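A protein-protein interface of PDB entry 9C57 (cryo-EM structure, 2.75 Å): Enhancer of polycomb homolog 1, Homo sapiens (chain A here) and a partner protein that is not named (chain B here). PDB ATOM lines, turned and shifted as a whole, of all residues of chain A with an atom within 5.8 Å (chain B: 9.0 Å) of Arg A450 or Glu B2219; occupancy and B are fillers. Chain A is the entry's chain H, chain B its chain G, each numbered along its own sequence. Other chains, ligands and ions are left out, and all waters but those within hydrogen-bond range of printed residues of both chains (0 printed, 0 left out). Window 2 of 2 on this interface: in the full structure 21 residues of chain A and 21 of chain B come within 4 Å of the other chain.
Tyr B2233 touches Thr A443.
Thr A444 touches Glu B2232 (O to O, 3.9 Å).
Thr A444 touches Tyr B2233 (N to CD2, 3.6 Å).
CB of Leu A445 touches OD2 of Asp B2227, 3.2 Å away.
N of Val A447 touches OD2 of Asp B2227, 3.6 Å away.
Arg A450 touches Leu B2220 (CD to CD1, 3.9 Å).
The backbone NH (N) of Thr A446 lies within hydrogen-bond range of the side-chain carboxylate (OD2) of Asp B2227, 2.6 Å away.
The guanidinium group (NH1) of Arg A450 lies within salt-bridge range of the side-chain carboxylate (OE2) of Glu B2219.
Of the 15 printed residues of chain B, 5 touch a printed residue of chain A.
Hydrophobic or aromatic side chains of chain B within 4 Å of the printed part of chain A: Leu B2220 and Tyr B2233.
Among the printed residues, Asp or Glu carboxylates within 4 Å of a Lys or Arg side-chain nitrogen of the other chain: Arg A450 with Glu B2219 (3.6 Å).
Of the printed residues of chain B, Thr A443 touches Tyr B2233.
Of the printed residues of chain B, Thr A444 touches Glu B2232 (3.9 Å) and Tyr B2233 (3.6 Å).
Printed residues of chain B within 4 Å of Thr A446: Asp B2227 (2.6 Å).
Arg A450 touches two residues of chain B.
Glu B2214 touches none of the printed residues of chain A.
Glu B2217 touches none of the printed residues of chain A.
Of the printed residues of chain A, Glu B2219 touches Arg A450.
Printed residues of chain A within 4 Å of Glu B2232: Thr A444 (3.9 Å).
Of the printed residues of chain A, Tyr B2233 touches Thr A443 (3.7 Å) and Thr A444 (3.6 Å).
The nearest residue of chain B that does not touch Arg A450 is Asp B2227 (7.5 Å).
The nearest printed residue of chain A that does not touch Glu B2219 is Ile A452 (6.0 Å).
O of Thr A443 lies within hydrogen-bond range of N of Ile A452 (3.0 Å).
N of Leu A445 lies within hydrogen-bond range of O of Arg A450, 3.4 Å away.
O of Pro A448 is in hydrogen-bond range of NE of Arg A450 (3.1 Å).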
ATOM      1  N   THR A 443      18.405   8.895  20.723  1.00  0.00           N
ATOM      2  CA  THR A 443      18.051   7.716  19.950  1.00  0.00           C
ATOM      3  C   THR A 443      18.742   6.495  20.534  1.00  0.00           C
ATOM      4  O   THR A 443      19.807   6.597  21.150  1.00  0.00           O
ATOM      5  CB  THR A 443      18.432   7.863  18.471  1.00  0.00           C
ATOM      6  OG1 THR A 443      19.857   7.833  18.335  1.00  0.00           O
ATOM      7  CG2 THR A 443      17.896   9.165  17.902  1.00  0.00           C
ATOM      8  N   THR A 444      18.118   5.338  20.337  1.00  0.00           N
ATOM      9  CA  THR A 444      18.656   4.056  20.770  1.00  0.00           C
ATOM     10  C   THR A 444      18.667   3.099  19.589  1.00  0.00           C
ATOM     11  O   THR A 444      17.631   2.881  18.952  1.00  0.00           O
ATOM     12  CB  THR A 444      17.831   3.457  21.910  1.00  0.00           C
ATOM     13  OG1 THR A 444      16.776   2.655  21.367  1.00  0.00           O
ATOM     14  CG2 THR A 444      17.234   4.554  22.780  1.00  0.00           C
ATOM     15  N   LEU A 445      19.833   2.531  19.302  1.00  0.00           N
ATOM     16  CA  LEU A 445      19.945   1.525  18.262  1.00  0.00           C
ATOM     17  C   LEU A 445      19.423   0.188  18.780  1.00  0.00           C
ATOM     18  O   LEU A 445      19.098   0.032  19.959  1.00  0.00           O
ATOM     19  CB  LEU A 445      21.396   1.396  17.801  1.00  0.00           C
ATOM     20  CG  LEU A 445      22.050   2.627  17.164  1.00  0.00           C
ATOM     21  CD1 LEU A 445      21.095   3.333  16.213  1.00  0.00           C
ATOM     22  CD2 LEU A 445      22.559   3.593  18.220  1.00  0.00           C
ATOM     23  N   THR A 446      19.337  -0.789  17.881  1.00  0.00           N
ATOM     24  CA  THR A 446      18.844  -2.113  18.244  1.00  0.00           C
ATOM     25  C   THR A 446      19.969  -3.126  18.404  1.00  0.00           C
ATOM     26  O   THR A 446      20.074  -3.770  19.450  1.00  0.00           O
ATOM     27  CB  THR A 446      17.844  -2.618  17.200  1.00  0.00           C
ATOM     28  OG1 THR A 446      18.491  -2.731  15.928  1.00  0.00           O
ATOM     29  CG2 THR A 446      16.666  -1.664  17.087  1.00  0.00           C
ATOM     30  N   VAL A 447      20.818  -3.282  17.392  1.00  0.00           N
ATOM     31  CA  VAL A 447      21.899  -4.260  17.467  1.00  0.00           C
ATOM     32  C   VAL A 447      22.906  -3.745  18.488  1.00  0.00           C
ATOM     33  O   VAL A 447      23.152  -4.418  19.498  1.00  0.00           O
ATOM     34  CB  VAL A 447      22.532  -4.511  16.090  1.00  0.00           C
ATOM     35  CG1 VAL A 447      23.992  -4.936  16.229  1.00  0.00           C
ATOM     36  CG2 VAL A 447      21.735  -5.568  15.343  1.00  0.00           C
ATOM     37  N   PRO A 448      23.509  -2.569  18.286  1.00  0.00           N
ATOM     38  CA  PRO A 448      24.262  -1.967  19.401  1.00  0.00           C
ATOM     39  C   PRO A 448      23.319  -1.232  20.346  1.00  0.00           C
ATOM     40  O   PRO A 448      23.247   0.000  20.394  1.00  0.00           O
ATOM     41  CB  PRO A 448      25.232  -1.034  18.673  1.00  0.00           C
ATOM     42  CG  PRO A 448      24.466  -0.583  17.480  1.00  0.00           C
ATOM     43  CD  PRO A 448      23.548  -1.717  17.084  1.00  0.00           C
ATOM     44  N   GLN A 449      22.570  -2.005  21.131  1.00  0.00           N
ATOM     45  CA  GLN A 449      21.437  -1.459  21.868  1.00  0.00           C
ATOM     46  C   GLN A 449      21.895  -0.545  22.995  1.00  0.00           C
ATOM     47  O   GLN A 449      22.152  -1.000  24.113  1.00  0.00           O
ATOM     48  CB  GLN A 449      20.577  -2.587  22.436  1.00  0.00           C
ATOM     49  CG  GLN A 449      19.270  -2.110  23.028  1.00  0.00           C
ATOM     50  CD  GLN A 449      19.107  -2.516  24.472  1.00  0.00           C
ATOM     51  OE1 GLN A 449      18.163  -3.220  24.826  1.00  0.00           O
ATOM     52  NE2 GLN A 449      20.035  -2.088  25.316  1.00  0.00           N
ATOM     53  N   ARG A 450      21.983   0.749  22.708  1.00  0.00           N
ATOM     54  CA  ARG A 450      22.363   1.729  23.710  1.00  0.00           C
ATOM     55  C   ARG A 450      21.865   3.092  23.259  1.00  0.00           C
ATOM     56  O   ARG A 450      21.610   3.317  22.074  1.00  0.00           O
ATOM     57  CB  ARG A 450      23.880   1.751  23.934  1.00  0.00           C
ATOM     58  CG  ARG A 450      24.660   2.558  22.892  1.00  0.00           C
ATOM     59  CD  ARG A 450      25.952   1.876  22.449  1.00  0.00           C
ATOM     60  NE  ARG A 450      25.764   0.478  22.080  1.00  0.00           N
ATOM     61  CZ  ARG A 450      26.746  -0.404  21.969  1.00  0.00           C
ATOM     62  NH1 ARG A 450      28.009  -0.060  22.152  1.00  0.00           N
ATOM     63  NH2 ARG A 450      26.455  -1.663  21.662  1.00  0.00           N
ATOM     64  N   CYS A 451      21.732   3.997  24.220  1.00  0.00           N
ATOM     65  CA  CYS A 451      21.333   5.364  23.924  1.00  0.00           C
ATOM     66  C   CYS A 451      22.547   6.137  23.425  1.00  0.00           C
ATOM     67  O   CYS A 451      23.417   6.516  24.216  1.00  0.00           O
ATOM     68  CB  CYS A 451      20.741   6.026  25.165  1.00  0.00           C
ATOM     69  SG  CYS A 451      19.522   5.011  26.027  1.00  0.00           S
ATOM     70  N   ILE A 452      22.608   6.371  22.113  1.00  0.00           N
ATOM     71  CA  ILE A 452      23.765   7.039  21.521  1.00  0.00           C
ATOM     72  C   ILE A 452      23.807   8.522  21.852  1.00  0.00           C
ATOM     73  O   ILE A 452      24.875   9.144  21.732  1.00  0.00           O
ATOM     74  CB  ILE A 452      23.778   6.835  19.991  1.00  0.00           C
ATOM     75  CG1 ILE A 452      24.921   7.612  19.333  1.00  0.00           C
ATOM     76  CG2 ILE A 452      22.455   7.266  19.381  1.00  0.00           C
ATOM     77  CD1 ILE A 452      26.289   7.259  19.865  1.00  0.00           C
ATOM     78  N   ALA B 835      37.574   9.898  11.020  1.00  0.00           N
ATOM     79  CA  ALA B 835      37.440   9.111  12.242  1.00  0.00           C
ATOM     80  C   ALA B 835      37.703   7.635  11.981  1.00  0.00           C
ATOM     81  O   ALA B 835      38.329   6.956  12.802  1.00  0.00           O
ATOM     82  CB  ALA B 835      36.054   9.308  12.842  1.00  0.00           C
ATOM     83  N   LYS B 839      40.580   5.343  13.641  1.00  0.00           N
ATOM     84  CA  LYS B 839      40.300   4.129  14.397  1.00  0.00           C
ATOM     85  C   LYS B 839      41.003   2.925  13.786  1.00  0.00           C
ATOM     86  O   LYS B 839      41.559   2.094  14.507  1.00  0.00           O
ATOM     87  CB  LYS B 839      38.794   3.889  14.470  1.00  0.00           C
ATOM     88  CG  LYS B 839      38.404   2.806  15.458  1.00  0.00           C
ATOM     89  CD  LYS B 839      36.901   2.658  15.564  1.00  0.00           C
ATOM     90  CE  LYS B 839      36.495   2.146  16.932  1.00  0.00           C
ATOM     91  NZ  LYS B 839      37.088   0.817  17.232  1.00  0.00           N
ATOM     92  N   THR B 843      43.906   0.783  15.482  1.00  0.00           N
ATOM     93  CA  THR B 843      43.724  -0.645  15.721  1.00  0.00           C
ATOM     94  C   THR B 843      44.851  -1.461  15.102  1.00  0.00           C
ATOM     95  O   THR B 843      45.249  -2.482  15.664  1.00  0.00           O
ATOM     96  CB  THR B 843      42.378  -1.115  15.169  1.00  0.00           C
ATOM     97  OG1 THR B 843      42.129  -0.491  13.906  1.00  0.00           O
ATOM     98  CG2 THR B 843      41.253  -0.777  16.129  1.00  0.00           C
ATOM     99  N   GLU B2214      42.021   3.445  24.813  1.00  0.00           N
ATOM    100  CA  GLU B2214      41.130   2.676  23.953  1.00  0.00           C
ATOM    101  C   GLU B2214      39.780   3.362  23.828  1.00  0.00           C
ATOM    102  O   GLU B2214      39.247   3.522  22.724  1.00  0.00           O
ATOM    103  CB  GLU B2214      40.952   1.266  24.513  1.00  0.00           C
ATOM    104  CG  GLU B2214      42.199   0.432  24.451  1.00  0.00           C
ATOM    105  CD  GLU B2214      42.610   0.154  23.038  1.00  0.00           C
ATOM    106  OE1 GLU B2214      41.909  -0.622  22.357  1.00  0.00           O
ATOM    107  OE2 GLU B2214      43.612   0.749  22.597  1.00  0.00           O
ATOM    108  N   GLN B2215      39.214   3.776  24.960  1.00  0.00           N
ATOM    109  CA  GLN B2215      37.915   4.433  24.933  1.00  0.00           C
ATOM    110  C   GLN B2215      37.965   5.702  24.096  1.00  0.00           C
ATOM    111  O   GLN B2215      36.943   6.117  23.541  1.00  0.00           O
ATOM    112  CB  GLN B2215      37.454   4.691  26.380  1.00  0.00           C
ATOM    113  CG  GLN B2215      36.195   5.567  26.638  1.00  0.00           C
ATOM    114  CD  GLN B2215      36.236   6.988  26.090  1.00  0.00           C
ATOM    115  OE1 GLN B2215      37.299   7.530  25.789  1.00  0.00           O
ATOM    116  NE2 GLN B2215      35.062   7.592  25.946  1.00  0.00           N
ATOM    117  N   GLU B2216      39.145   6.313  23.963  1.00  0.00           N
ATOM    118  CA  GLU B2216      39.221   7.598  23.274  1.00  0.00           C
ATOM    119  C   GLU B2216      38.686   7.507  21.847  1.00  0.00           C
ATOM    120  O   GLU B2216      37.953   8.394  21.397  1.00  0.00           O
ATOM    121  CB  GLU B2216      40.661   8.121  23.280  1.00  0.00           C
ATOM    122  CG  GLU B2216      41.389   8.036  21.948  1.00  0.00           C
ATOM    123  CD  GLU B2216      42.849   8.403  22.066  1.00  0.00           C
ATOM    124  OE1 GLU B2216      43.145   9.588  22.323  1.00  0.00           O
ATOM    125  OE2 GLU B2216      43.704   7.508  21.900  1.00  0.00           O
ATOM    126  N   GLU B2217      39.034   6.450  21.120  1.00  0.00           N
ATOM    127  CA  GLU B2217      38.596   6.330  19.737  1.00  0.00           C
ATOM    128  C   GLU B2217      37.090   6.123  19.666  1.00  0.00           C
ATOM    129  O   GLU B2217      36.484   5.491  20.535  1.00  0.00           O
ATOM    130  CB  GLU B2217      39.310   5.171  19.043  1.00  0.00           C
ATOM    131  CG  GLU B2217      40.730   5.488  18.615  1.00  0.00           C
ATOM    132  CD  GLU B2217      41.703   4.394  18.997  1.00  0.00           C
ATOM    133  OE1 GLU B2217      41.332   3.208  18.902  1.00  0.00           O
ATOM    134  OE2 GLU B2217      42.833   4.718  19.413  1.00  0.00           O
ATOM    135  N   ALA B2218      36.484   6.657  18.607  1.00  0.00           N
ATOM    136  CA  ALA B2218      35.041   6.562  18.438  1.00  0.00           C
ATOM    137  C   ALA B2218      34.624   5.103  18.356  1.00  0.00           C
ATOM    138  O   ALA B2218      34.884   4.432  17.354  1.00  0.00           O
ATOM    139  CB  ALA B2218      34.595   7.316  17.185  1.00  0.00           C
ATOM    140  N   GLU B2219      33.958   4.610  19.399  1.00  0.00           N
ATOM    141  CA  GLU B2219      33.676   3.182  19.480  1.00  0.00           C
ATOM    142  C   GLU B2219      32.743   2.722  18.368  1.00  0.00           C
ATOM    143  O   GLU B2219      32.817   1.564  17.941  1.00  0.00           O
ATOM    144  CB  GLU B2219      33.080   2.843  20.846  1.00  0.00           C
ATOM    145  CG  GLU B2219      31.822   3.616  21.191  1.00  0.00           C
ATOM    146  CD  GLU B2219      31.046   2.979  22.325  1.00  0.00           C
ATOM    147  OE1 GLU B2219      31.679   2.353  23.200  1.00  0.00           O
ATOM    148  OE2 GLU B2219      29.804   3.106  22.342  1.00  0.00           O
ATOM    149  N   LEU B2220      31.869   3.600  17.884  1.00  0.00           N
ATOM    150  CA  LEU B2220      30.854   3.231  16.907  1.00  0.00           C
ATOM    151  C   LEU B2220      31.054   4.030  15.629  1.00  0.00           C
ATOM    152  O   LEU B2220      31.143   5.261  15.669  1.00  0.00           O
ATOM    153  CB  LEU B2220      29.450   3.469  17.462  1.00  0.00           C
ATOM    154  CG  LEU B2220      28.982   2.471  18.522  1.00  0.00           C
ATOM    155  CD1 LEU B2220      27.660   2.913  19.114  1.00  0.00           C
ATOM    156  CD2 LEU B2220      28.860   1.077  17.937  1.00  0.00           C
ATOM    157  N   LEU B2221      31.125   3.327  14.502  1.00  0.00           N
ATOM    158  CA  LEU B2221      31.207   3.953  13.191  1.00  0.00           C
ATOM    159  C   LEU B2221      30.059   3.587  12.266  1.00  0.00           C
ATOM    160  O   LEU B2221      29.704   4.396  11.408  1.00  0.00           O
ATOM    161  CB  LEU B2221      32.525   3.581  12.495  1.00  0.00           C
ATOM    162  CG  LEU B2221      33.811   4.122  13.117  1.00  0.00           C
ATOM    163  CD1 LEU B2221      35.017   3.564  12.388  1.00  0.00           C
ATOM    164  CD2 LEU B2221      33.827   5.639  13.094  1.00  0.00           C
ATOM    165  N   THR B2222      29.477   2.400  12.406  1.00  0.00           N
ATOM    166  CA  THR B2222      28.395   1.948  11.544  1.00  0.00           C
ATOM    167  C   THR B2222      27.320   1.291  12.399  1.00  0.00           C
ATOM    168  O   THR B2222      27.481   1.115  13.609  1.00  0.00           O
ATOM    169  CB  THR B2222      28.910   0.976  10.473  1.00  0.00           C
ATOM    170  OG1 THR B2222      29.272  -0.267  11.084  1.00  0.00           O
ATOM    171  CG2 THR B2222      30.119   1.553   9.759  1.00  0.00           C
ATOM    172  N   ASP B2227      18.517  -2.168  11.331  1.00  0.00           N
ATOM    173  CA  ASP B2227      18.421  -1.094  12.311  1.00  0.00           C
ATOM    174  C   ASP B2227      18.650   0.266  11.666  1.00  0.00           C
ATOM    175  O   ASP B2227      18.971   1.237  12.357  1.00  0.00           O
ATOM    176  CB  ASP B2227      19.423  -1.319  13.444  1.00  0.00           C
ATOM    177  CG  ASP B2227      19.207  -0.380  14.607  1.00  0.00           C
ATOM    178  OD1 ASP B2227      18.148   0.277  14.653  1.00  0.00           O
ATOM    179  OD2 ASP B2227      20.094  -0.301  15.482  1.00  0.00           O
ATOM    180  N   GLU B2232      13.268   2.110  13.543  1.00  0.00           N
ATOM    181  CA  GLU B2232      14.177   1.801  14.642  1.00  0.00           C
ATOM    182  C   GLU B2232      13.847   2.441  15.991  1.00  0.00           C
ATOM    183  O   GLU B2232      14.351   1.977  17.019  1.00  0.00           O
ATOM    184  CB  GLU B2232      15.598   2.215  14.255  1.00  0.00           C
ATOM    185  CG  GLU B2232      15.918   2.088  12.774  1.00  0.00           C
ATOM    186  CD  GLU B2232      15.534   0.739  12.199  1.00  0.00           C
ATOM    187  OE1 GLU B2232      15.293  -0.203  12.981  1.00  0.00           O
ATOM    188  OE2 GLU B2232      15.484   0.617  10.959  1.00  0.00           O
ATOM    189  N   TYR B2233      13.000   3.474  16.020  1.00  0.00           N
ATOM    190  CA  TYR B2233      12.828   4.255  17.243  1.00  0.00           C
ATOM    191  C   TYR B2233      11.929   5.467  17.011  1.00  0.00           C
ATOM    192  O   TYR B2233      11.770   5.918  15.873  1.00  0.00           O
ATOM    193  CB  TYR B2233      14.215   4.649  17.786  1.00  0.00           C
ATOM    194  CG  TYR B2233      14.277   5.798  18.769  1.00  0.00           C
ATOM    195  CD1 TYR B2233      14.099   7.111  18.356  1.00  0.00           C
ATOM    196  CD2 TYR B2233      14.505   5.565  20.118  1.00  0.00           C
ATOM    197  CE1 TYR B2233      14.165   8.155  19.249  1.00  0.00           C
ATOM    198  CE2 TYR B2233      14.562   6.605  21.023  1.00  0.00           C
ATOM    199  CZ  TYR B2233      14.385   7.898  20.583  1.00  0.00           C
ATOM    200  OH  TYR B2233      14.444   8.945  21.474  1.00  0.00           O
